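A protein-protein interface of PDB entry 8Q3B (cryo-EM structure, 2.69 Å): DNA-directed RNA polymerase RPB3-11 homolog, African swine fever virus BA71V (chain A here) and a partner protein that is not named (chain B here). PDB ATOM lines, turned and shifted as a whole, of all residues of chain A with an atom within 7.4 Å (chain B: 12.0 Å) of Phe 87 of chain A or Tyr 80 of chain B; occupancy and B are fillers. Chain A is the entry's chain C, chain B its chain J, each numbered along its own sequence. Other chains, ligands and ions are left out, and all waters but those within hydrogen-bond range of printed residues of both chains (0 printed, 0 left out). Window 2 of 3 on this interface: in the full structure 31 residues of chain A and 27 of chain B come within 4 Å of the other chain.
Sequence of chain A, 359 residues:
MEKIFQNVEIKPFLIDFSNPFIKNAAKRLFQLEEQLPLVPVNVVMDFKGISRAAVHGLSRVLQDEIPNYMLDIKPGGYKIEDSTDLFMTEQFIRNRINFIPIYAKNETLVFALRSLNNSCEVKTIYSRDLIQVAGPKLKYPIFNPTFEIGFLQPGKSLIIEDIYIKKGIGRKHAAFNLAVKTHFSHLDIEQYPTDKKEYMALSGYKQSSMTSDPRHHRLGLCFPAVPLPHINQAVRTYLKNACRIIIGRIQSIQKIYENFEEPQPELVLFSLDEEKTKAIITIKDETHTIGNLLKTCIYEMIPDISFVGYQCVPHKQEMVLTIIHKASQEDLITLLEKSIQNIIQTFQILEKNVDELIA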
ATOM      1  N   TYR A  78     -11.397 -26.518  12.539  1.00  0.00           N
ATOM      2  CA  TYR A  78      -9.995 -26.693  12.897  1.00  0.00           C
ATOM      3  C   TYR A  78      -9.495 -27.995  12.286  1.00  0.00           C
ATOM      4  O   TYR A  78      -9.839 -29.084  12.759  1.00  0.00           O
ATOM      5  CB  TYR A  78      -9.828 -26.695  14.412  1.00  0.00           C
ATOM      6  CG  TYR A  78      -8.390 -26.713  14.875  1.00  0.00           C
ATOM      7  CD1 TYR A  78      -7.703 -27.908  15.028  1.00  0.00           C
ATOM      8  CD2 TYR A  78      -7.721 -25.532  15.165  1.00  0.00           C
ATOM      9  CE1 TYR A  78      -6.390 -27.926  15.454  1.00  0.00           C
ATOM     10  CE2 TYR A  78      -6.410 -25.541  15.591  1.00  0.00           C
ATOM     11  CZ  TYR A  78      -5.748 -26.740  15.734  1.00  0.00           C
ATOM     12  OH  TYR A  78      -4.440 -26.751  16.157  1.00  0.00           O
ATOM     13  N   THR A  84       0.410 -29.631  12.061  1.00  0.00           N
ATOM     14  CA  THR A  84      -0.259 -28.732  12.992  1.00  0.00           C
ATOM     15  C   THR A  84       0.571 -28.558  14.256  1.00  0.00           C
ATOM     16  O   THR A  84       1.091 -29.525  14.820  1.00  0.00           O
ATOM     17  CB  THR A  84      -1.648 -29.260  13.346  1.00  0.00           C
ATOM     18  OG1 THR A  84      -1.588 -30.674  13.565  1.00  0.00           O
ATOM     19  CG2 THR A  84      -2.632 -28.953  12.228  1.00  0.00           C
ATOM     20  N   ASP A  85       0.694 -27.310  14.701  1.00  0.00           N
ATOM     21  CA  ASP A  85       1.496 -27.010  15.878  1.00  0.00           C
ATOM     22  C   ASP A  85       0.862 -27.610  17.126  1.00  0.00           C
ATOM     23  O   ASP A  85      -0.361 -27.605  17.286  1.00  0.00           O
ATOM     24  CB  ASP A  85       1.653 -25.499  16.042  1.00  0.00           C
ATOM     25  CG  ASP A  85       2.739 -25.132  17.033  1.00  0.00           C
ATOM     26  OD1 ASP A  85       3.399 -26.050  17.559  1.00  0.00           O
ATOM     27  OD2 ASP A  85       2.932 -23.924  17.285  1.00  0.00           O
ATOM     28  N   LEU A  86       1.709 -28.131  18.014  1.00  0.00           N
ATOM     29  CA  LEU A  86       1.208 -28.769  19.227  1.00  0.00           C
ATOM     30  C   LEU A  86       0.691 -27.741  20.225  1.00  0.00           C
ATOM     31  O   LEU A  86      -0.354 -27.947  20.852  1.00  0.00           O
ATOM     32  CB  LEU A  86       2.310 -29.616  19.861  1.00  0.00           C
ATOM     33  CG  LEU A  86       3.027 -30.601  18.934  1.00  0.00           C
ATOM     34  CD1 LEU A  86       3.977 -31.479  19.732  1.00  0.00           C
ATOM     35  CD2 LEU A  86       2.033 -31.453  18.159  1.00  0.00           C
ATOM     36  N   PHE A  87       1.410 -26.629  20.389  1.00  0.00           N
ATOM     37  CA  PHE A  87       1.037 -25.651  21.406  1.00  0.00           C
ATOM     38  C   PHE A  87      -0.271 -24.953  21.058  1.00  0.00           C
ATOM     39  O   PHE A  87      -1.111 -24.725  21.937  1.00  0.00           O
ATOM     40  CB  PHE A  87       2.159 -24.629  21.581  1.00  0.00           C
ATOM     41  CG  PHE A  87       3.478 -25.241  21.946  1.00  0.00           C
ATOM     42  CD1 PHE A  87       3.692 -25.744  23.217  1.00  0.00           C
ATOM     43  CD2 PHE A  87       4.501 -25.321  21.019  1.00  0.00           C
ATOM     44  CE1 PHE A  87       4.903 -26.311  23.558  1.00  0.00           C
ATOM     45  CE2 PHE A  87       5.714 -25.885  21.354  1.00  0.00           C
ATOM     46  CZ  PHE A  87       5.915 -26.381  22.624  1.00  0.00           C
ATOM     47  N   MET A  88      -0.467 -24.604  19.786  1.00  0.00           N
ATOM     48  CA  MET A  88      -1.663 -23.883  19.355  1.00  0.00           C
ATOM     49  C   MET A  88      -2.827 -24.867  19.229  1.00  0.00           C
ATOM     50  O   MET A  88      -3.268 -25.241  18.140  1.00  0.00           O
ATOM     51  CB  MET A  88      -1.401 -23.155  18.044  1.00  0.00           C
ATOM     52  CG  MET A  88      -0.326 -22.081  18.132  1.00  0.00           C
ATOM     53  SD  MET A  88      -0.658 -20.851  19.407  1.00  0.00           S
ATOM     54  CE  MET A  88       0.781 -21.048  20.449  1.00  0.00           C
ATOM     55  N   THR A  89      -3.329 -25.287  20.388  1.00  0.00           N
ATOM     56  CA  THR A  89      -4.461 -26.197  20.426  1.00  0.00           C
ATOM     57  C   THR A  89      -5.734 -25.472  19.994  1.00  0.00           C
ATOM     58  O   THR A  89      -5.794 -24.241  19.933  1.00  0.00           O
ATOM     59  CB  THR A  89      -4.639 -26.782  21.828  1.00  0.00           C
ATOM     60  OG1 THR A  89      -5.177 -25.782  22.703  1.00  0.00           O
ATOM     61  CG2 THR A  89      -3.313 -27.285  22.382  1.00  0.00           C
ATOM     62  N   GLU A  90      -6.765 -26.259  19.686  1.00  0.00           N
ATOM     63  CA  GLU A  90      -8.020 -25.672  19.231  1.00  0.00           C
ATOM     64  C   GLU A  90      -8.659 -24.816  20.315  1.00  0.00           C
ATOM     65  O   GLU A  90      -9.244 -23.770  20.019  1.00  0.00           O
ATOM     66  CB  GLU A  90      -8.986 -26.765  18.779  1.00  0.00           C
ATOM     67  CG  GLU A  90     -10.165 -26.235  17.977  1.00  0.00           C
ATOM     68  CD  GLU A  90     -11.311 -27.222  17.892  1.00  0.00           C
ATOM     69  OE1 GLU A  90     -11.208 -28.311  18.494  1.00  0.00           O
ATOM     70  OE2 GLU A  90     -12.317 -26.906  17.223  1.00  0.00           O
ATOM     71  N   PHE A  92      -7.175 -23.048  22.699  1.00  0.00           N
ATOM     72  CA  PHE A  92      -6.460 -21.780  22.811  1.00  0.00           C
ATOM     73  C   PHE A  92      -6.834 -20.838  21.672  1.00  0.00           C
ATOM     74  O   PHE A  92      -7.164 -19.667  21.900  1.00  0.00           O
ATOM     75  CB  PHE A  92      -4.954 -22.042  22.822  1.00  0.00           C
ATOM     76  CG  PHE A  92      -4.126 -20.828  23.126  1.00  0.00           C
ATOM     77  CD1 PHE A  92      -4.134 -20.264  24.388  1.00  0.00           C
ATOM     78  CD2 PHE A  92      -3.331 -20.255  22.150  1.00  0.00           C
ATOM     79  CE1 PHE A  92      -3.370 -19.151  24.668  1.00  0.00           C
ATOM     80  CE2 PHE A  92      -2.567 -19.142  22.425  1.00  0.00           C
ATOM     81  CZ  PHE A  92      -2.586 -18.590  23.685  1.00  0.00           C
ATOM     82  N   ILE A  93      -6.795 -21.335  20.436  1.00  0.00           N
ATOM     83  CA  ILE A  93      -7.074 -20.481  19.288  1.00  0.00           C
ATOM     84  C   ILE A  93      -8.531 -20.039  19.294  1.00  0.00           C
ATOM     85  O   ILE A  93      -8.848 -18.900  18.935  1.00  0.00           O
ATOM     86  CB  ILE A  93      -6.708 -21.206  17.981  1.00  0.00           C
ATOM     87  CG1 ILE A  93      -5.221 -21.571  17.968  1.00  0.00           C
ATOM     88  CG2 ILE A  93      -7.055 -20.342  16.780  1.00  0.00           C
ATOM     89  CD1 ILE A  93      -4.284 -20.378  17.910  1.00  0.00           C
ATOM     90  N   VAL A 122      10.439 -18.966  15.236  1.00  0.00           N
ATOM     91  CA  VAL A 122       9.027 -18.915  15.587  1.00  0.00           C
ATOM     92  C   VAL A 122       8.372 -17.750  14.863  1.00  0.00           C
ATOM     93  O   VAL A 122       8.850 -16.610  14.922  1.00  0.00           O
ATOM     94  CB  VAL A 122       8.861 -18.792  17.110  1.00  0.00           C
ATOM     95  CG1 VAL A 122       7.441 -18.376  17.465  1.00  0.00           C
ATOM     96  CG2 VAL A 122       9.226 -20.099  17.791  1.00  0.00           C
ATOM     97  N   PHE A 151       1.273 -18.095  17.756  1.00  0.00           N
ATOM     98  CA  PHE A 151       2.616 -18.259  17.220  1.00  0.00           C
ATOM     99  C   PHE A 151       2.843 -19.720  16.859  1.00  0.00           C
ATOM    100  O   PHE A 151       2.262 -20.625  17.462  1.00  0.00           O
ATOM    101  CB  PHE A 151       3.689 -17.782  18.207  1.00  0.00           C
ATOM    102  CG  PHE A 151       3.622 -18.447  19.549  1.00  0.00           C
ATOM    103  CD1 PHE A 151       2.777 -17.968  20.534  1.00  0.00           C
ATOM    104  CD2 PHE A 151       4.413 -19.547  19.830  1.00  0.00           C
ATOM    105  CE1 PHE A 151       2.718 -18.577  21.769  1.00  0.00           C
ATOM    106  CE2 PHE A 151       4.357 -20.159  21.064  1.00  0.00           C
ATOM    107  CZ  PHE A 151       3.509 -19.673  22.034  1.00  0.00           C
ATOM    108  N   LEU A 152       3.702 -19.932  15.864  1.00  0.00           N
ATOM    109  CA  LEU A 152       4.004 -21.248  15.324  1.00  0.00           C
ATOM    110  C   LEU A 152       5.498 -21.521  15.407  1.00  0.00           C
ATOM    111  O   LEU A 152       6.319 -20.643  15.114  1.00  0.00           O
ATOM    112  CB  LEU A 152       3.553 -21.366  13.866  1.00  0.00           C
ATOM    113  CG  LEU A 152       2.075 -21.105  13.600  1.00  0.00           C
ATOM    114  CD1 LEU A 152       1.813 -21.008  12.108  1.00  0.00           C
ATOM    115  CD2 LEU A 152       1.218 -22.191  14.227  1.00  0.00           C
ATOM    116  N   GLN A 153       5.838 -22.745  15.802  1.00  0.00           N
ATOM    117  CA  GLN A 153       7.217 -23.193  15.789  1.00  0.00           C
ATOM    118  C   GLN A 153       7.664 -23.449  14.352  1.00  0.00           C
ATOM    119  O   GLN A 153       6.835 -23.655  13.464  1.00  0.00           O
ATOM    120  CB  GLN A 153       7.369 -24.464  16.622  1.00  0.00           C
ATOM    121  CG  GLN A 153       6.744 -24.385  18.007  1.00  0.00           C
ATOM    122  CD  GLN A 153       7.509 -23.467  18.936  1.00  0.00           C
ATOM    123  OE1 GLN A 153       8.657 -23.112  18.672  1.00  0.00           O
ATOM    124  NE2 GLN A 153       6.874 -23.074  20.033  1.00  0.00           N
ATOM    125  N   LYS A 156       5.919 -25.775  11.351  1.00  0.00           N
ATOM    126  CA  LYS A 156       4.545 -26.084  11.715  1.00  0.00           C
ATOM    127  C   LYS A 156       3.576 -25.199  10.939  1.00  0.00           C
ATOM    128  O   LYS A 156       3.966 -24.255  10.249  1.00  0.00           O
ATOM    129  CB  LYS A 156       4.337 -25.909  13.221  1.00  0.00           C
ATOM    130  CG  LYS A 156       5.240 -26.781  14.079  1.00  0.00           C
ATOM    131  CD  LYS A 156       4.810 -28.236  14.044  1.00  0.00           C
ATOM    132  CE  LYS A 156       6.006 -29.166  13.958  1.00  0.00           C
ATOM    133  NZ  LYS A 156       5.634 -30.583  14.220  1.00  0.00           N
ATOM    134  N   LEU A 158      -0.941 -23.907  10.832  1.00  0.00           N
ATOM    135  CA  LEU A 158      -2.255 -23.832  11.462  1.00  0.00           C
ATOM    136  C   LEU A 158      -3.285 -23.528  10.387  1.00  0.00           C
ATOM    137  O   LEU A 158      -3.150 -22.541   9.656  1.00  0.00           O
ATOM    138  CB  LEU A 158      -2.285 -22.763  12.559  1.00  0.00           C
ATOM    139  CG  LEU A 158      -3.561 -22.708  13.401  1.00  0.00           C
ATOM    140  CD1 LEU A 158      -3.481 -23.690  14.558  1.00  0.00           C
ATOM    141  CD2 LEU A 158      -3.805 -21.299  13.912  1.00  0.00           C
ATOM    142  N   MET B   1       0.201 -17.806  27.240  1.00  0.00           N
ATOM    143  CA  MET B   1       1.335 -17.823  26.275  1.00  0.00           C
ATOM    144  C   MET B   1       1.583 -16.435  25.703  1.00  0.00           C
ATOM    145  O   MET B   1       2.704 -16.096  25.329  1.00  0.00           O
ATOM    146  CB  MET B   1       1.059 -18.805  25.137  1.00  0.00           C
ATOM    147  CG  MET B   1       0.549 -20.157  25.589  1.00  0.00           C
ATOM    148  SD  MET B   1       1.069 -21.481  24.485  1.00  0.00           S
ATOM    149  CE  MET B   1      -0.260 -22.653  24.723  1.00  0.00           C
ATOM    150  N   LEU B   2       0.521 -15.637  25.634  1.00  0.00           N
ATOM    151  CA  LEU B   2       0.584 -14.297  25.075  1.00  0.00           C
ATOM    152  C   LEU B   2      -0.253 -13.368  25.940  1.00  0.00           C
ATOM    153  O   LEU B   2      -1.004 -13.806  26.814  1.00  0.00           O
ATOM    154  CB  LEU B   2       0.080 -14.266  23.626  1.00  0.00           C
ATOM    155  CG  LEU B   2       0.771 -15.208  22.641  1.00  0.00           C
ATOM    156  CD1 LEU B   2      -0.122 -15.475  21.444  1.00  0.00           C
ATOM    157  CD2 LEU B   2       2.099 -14.629  22.194  1.00  0.00           C
ATOM    158  N   ASP B  22       4.864  -4.759  23.581  1.00  0.00           N
ATOM    159  CA  ASP B  22       5.988  -5.638  23.880  1.00  0.00           C
ATOM    160  C   ASP B  22       7.244  -5.176  23.160  1.00  0.00           C
ATOM    161  O   ASP B  22       8.358  -5.346  23.668  1.00  0.00           O
ATOM    162  CB  ASP B  22       5.647  -7.079  23.500  1.00  0.00           C
ATOM    163  CG  ASP B  22       6.053  -8.078  24.570  1.00  0.00           C
ATOM    164  OD1 ASP B  22       6.798  -7.699  25.498  1.00  0.00           O
ATOM    165  OD2 ASP B  22       5.624  -9.247  24.482  1.00  0.00           O
ATOM    166  N   THR B  73       1.736 -10.026  32.208  1.00  0.00           N
ATOM    167  CA  THR B  73       1.510 -11.271  31.487  1.00  0.00           C
ATOM    168  C   THR B  73       2.816 -11.812  30.916  1.00  0.00           C
ATOM    169  O   THR B  73       3.652 -11.059  30.409  1.00  0.00           O
ATOM    170  CB  THR B  73       0.501 -11.068  30.360  1.00  0.00           C
ATOM    171  OG1 THR B  73      -0.593 -10.273  30.831  1.00  0.00           O
ATOM    172  CG2 THR B  73      -0.023 -12.410  29.881  1.00  0.00           C
ATOM    173  N   LEU B  74       2.982 -13.129  31.001  1.00  0.00           N
ATOM    174  CA  LEU B  74       4.173 -13.797  30.498  1.00  0.00           C
ATOM    175  C   LEU B  74       3.996 -14.151  29.028  1.00  0.00           C
ATOM    176  O   LEU B  74       2.887 -14.456  28.579  1.00  0.00           O
ATOM    177  CB  LEU B  74       4.460 -15.067  31.301  1.00  0.00           C
ATOM    178  CG  LEU B  74       4.870 -14.886  32.764  1.00  0.00           C
ATOM    179  CD1 LEU B  74       5.229 -16.228  33.372  1.00  0.00           C
ATOM    180  CD2 LEU B  74       6.021 -13.907  32.906  1.00  0.00           C
ATOM    181  N   ASP B  75       5.096 -14.111  28.284  1.00  0.00           N
ATOM    182  CA  ASP B  75       5.111 -14.454  26.869  1.00  0.00           C
ATOM    183  C   ASP B  75       5.856 -15.770  26.697  1.00  0.00           C
ATOM    184  O   ASP B  75       7.004 -15.899  27.133  1.00  0.00           O
ATOM    185  CB  ASP B  75       5.768 -13.346  26.046  1.00  0.00           C
ATOM    186  CG  ASP B  75       5.420 -13.430  24.575  1.00  0.00           C
ATOM    187  OD1 ASP B  75       4.768 -14.415  24.173  1.00  0.00           O
ATOM    188  OD2 ASP B  75       5.798 -12.509  23.821  1.00  0.00           O
ATOM    189  N   TYR B  76       5.200 -16.744  26.060  1.00  0.00           N
ATOM    190  CA  TYR B  76       5.810 -18.059  25.899  1.00  0.00           C
ATOM    191  C   TYR B  76       7.000 -18.017  24.952  1.00  0.00           C
ATOM    192  O   TYR B  76       7.926 -18.824  25.089  1.00  0.00           O
ATOM    193  CB  TYR B  76       4.771 -19.056  25.388  1.00  0.00           C
ATOM    194  CG  TYR B  76       5.016 -20.480  25.826  1.00  0.00           C
ATOM    195  CD1 TYR B  76       4.837 -20.860  27.149  1.00  0.00           C
ATOM    196  CD2 TYR B  76       5.423 -21.447  24.917  1.00  0.00           C
ATOM    197  CE1 TYR B  76       5.057 -22.162  27.553  1.00  0.00           C
ATOM    198  CE2 TYR B  76       5.646 -22.751  25.313  1.00  0.00           C
ATOM    199  CZ  TYR B  76       5.461 -23.102  26.631  1.00  0.00           C
ATOM    200  OH  TYR B  76       5.682 -24.399  27.032  1.00  0.00           O
ATOM    201  N   ARG B  77       6.997 -17.094  23.990  1.00  0.00           N
ATOM    202  CA  ARG B  77       8.104 -17.014  23.044  1.00  0.00           C
ATOM    203  C   ARG B  77       9.420 -16.750  23.764  1.00  0.00           C
ATOM    204  O   ARG B  77      10.446 -17.360  23.444  1.00  0.00           O
ATOM    205  CB  ARG B  77       7.833 -15.918  22.014  1.00  0.00           C
ATOM    206  CG  ARG B  77       6.917 -16.344  20.873  1.00  0.00           C
ATOM    207  CD  ARG B  77       5.507 -15.780  21.007  1.00  0.00           C
ATOM    208  NE  ARG B  77       5.493 -14.339  21.248  1.00  0.00           N
ATOM    209  CZ  ARG B  77       4.935 -13.436  20.449  1.00  0.00           C
ATOM    210  NH1 ARG B  77       4.330 -13.779  19.324  1.00  0.00           N
ATOM    211  NH2 ARG B  77       4.986 -12.153  20.792  1.00  0.00           N
ATOM    212  N   LYS B  78       9.409 -15.843  24.740  1.00  0.00           N
ATOM    213  CA  LYS B  78      10.634 -15.519  25.462  1.00  0.00           C
ATOM    214  C   LYS B  78      11.101 -16.690  26.318  1.00  0.00           C
ATOM    215  O   LYS B  78      12.292 -17.017  26.336  1.00  0.00           O
ATOM    216  CB  LYS B  78      10.412 -14.278  26.325  1.00  0.00           C
ATOM    217  CG  LYS B  78      10.007 -13.048  25.532  1.00  0.00           C
ATOM    218  CD  LYS B  78       9.562 -11.916  26.439  1.00  0.00           C
ATOM    219  CE  LYS B  78       9.357 -10.631  25.656  1.00  0.00           C
ATOM    220  NZ  LYS B  78       8.927  -9.504  26.527  1.00  0.00           N
ATOM    221  N   TYR B  79      10.177 -17.332  27.036  1.00  0.00           N
ATOM    222  CA  TYR B  79      10.565 -18.412  27.938  1.00  0.00           C
ATOM    223  C   TYR B  79      10.942 -19.672  27.170  1.00  0.00           C
ATOM    224  O   TYR B  79      11.945 -20.322  27.486  1.00  0.00           O
ATOM    225  CB  TYR B  79       9.431 -18.702  28.920  1.00  0.00           C
ATOM    226  CG  TYR B  79       9.499 -17.871  30.179  1.00  0.00           C
ATOM    227  CD1 TYR B  79      10.292 -18.259  31.249  1.00  0.00           C
ATOM    228  CD2 TYR B  79       8.773 -16.695  30.295  1.00  0.00           C
ATOM    229  CE1 TYR B  79      10.359 -17.500  32.401  1.00  0.00           C
ATOM    230  CE2 TYR B  79       8.834 -15.930  31.442  1.00  0.00           C
ATOM    231  CZ  TYR B  79       9.627 -16.337  32.492  1.00  0.00           C
ATOM    232  OH  TYR B  79       9.690 -15.577  33.638  1.00  0.00           O
ATOM    233  N   TYR B  80      10.156 -20.033  26.160  1.00  0.00           N
ATOM    234  CA  TYR B  80      10.398 -21.252  25.396  1.00  0.00           C
ATOM    235  C   TYR B  80      11.105 -20.918  24.088  1.00  0.00           C
ATOM    236  O   TYR B  80      12.287 -21.216  23.915  1.00  0.00           O
ATOM    237  CB  TYR B  80       9.075 -21.981  25.130  1.00  0.00           C
ATOM    238  CG  TYR B  80       9.208 -23.290  24.378  1.00  0.00           C
ATOM    239  CD1 TYR B  80       9.499 -23.315  23.019  1.00  0.00           C
ATOM    240  CD2 TYR B  80       9.037 -24.504  25.030  1.00  0.00           C
ATOM    241  CE1 TYR B  80       9.617 -24.509  22.335  1.00  0.00           C
ATOM    242  CE2 TYR B  80       9.154 -25.703  24.354  1.00  0.00           C
ATOM    243  CZ  TYR B  80       9.444 -25.700  23.007  1.00  0.00           C
ATOM    244  OH  TYR B  80       9.562 -26.892  22.329  1.00  0.00           O
ATOM    245  OXT TYR B  80      10.515 -20.343  23.175  1.00  0.00           O
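Phe 87 of chain A touches Met 1 of chain B.
CZ of Tyr 80 of chain B touches CZ of Phe 87 of chain A, at 3.6 Å.
Phe 92 of chain A touches Met 1 of chain B.
Phe 151 of chain A touches Met 1 of chain B (CE1 to CB, 3.8 Å).
CD2 of Leu 2 of chain B touches CD1 of Phe 151 of chain A, 3.8 Å away.
Phe 151 of chain A touches Tyr 76 of chain B (CZ to CB, 3.6 Å).
Arg 77 of chain B touches Phe 151 of chain A (CD to CD1, 3.5 Å).
Gln 153 of chain A touches Tyr 80 of chain B (NE2 to CE1, 3.9 Å).
No residue of chain B comes within 4 Å of Asp 85 of chain A.
Phe 87 of chain A touches just these residues of chain B: Met 1 and Tyr 80.
No residue of chain B comes within 4 Å of Met 88 of chain A.
No residue of chain B comes within 4 Å of Thr 89 of chain A.
Of chain B, only Met 1 comes within 4 Å of Phe 92 of chain A.
Phe 151 of chain A touches four residues of chain B.
Of the printed residues of chain B, Gln 153 of chain A touches Tyr 80 (3.9 Å).
Printed residues of chain A within 4 Å of Met 1 of chain B: Phe 87 (3.6 Å), Phe 92 (3.9 Å) and Phe 151 (3.8 Å).
Of the printed residues of chain A, Tyr 76 of chain B touches Phe 151.
Printed residues of chain A within 4 Å of Arg 77 of chain B: Phe 151.
Tyr 80 of chain B touches just these residues of chain A: Phe 87 and Gln 153.
Hydrophobic or aromatic side chains of chain B within 4 Å of the printed part of chain A: Met 1, Leu 2, Tyr 76 and Tyr 80.
Printed residues of chain A that touch a printed residue of chain B: Phe 87, Phe 92, Phe 151 and Gln 153.
Hydrophobic or aromatic side chains of chain A that line the printed part of chain B: Phe 87, Phe 92 and Phe 151.
Among the printed residues, 8 pairs touch across the chains.
OD2 of Asp 85 of chain A lies within hydrogen-bond range of N of Gln 153 of chain A (3.5 Å).
The side-chain sulfur (SD) of Met 88 of chain A lies within hydrogen-bond range of the backbone NH (N) of Phe 151 of chain A.
N of Phe 92 of chain A sits at hydrogen-bond distance from OG1 of Thr 89 of chain A.
The backbone NH (N) of Tyr 76 of chain B is in hydrogen-bond range of the backbone carbonyl oxygen (O) of Met 1 of chain B (2.7 Å).
The side-chain carboxylate (OD1) of Asp 75 of chain B lies within salt-bridge range of the guanidinium group (NE) of Arg 77 of chain B (3.0 Å).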
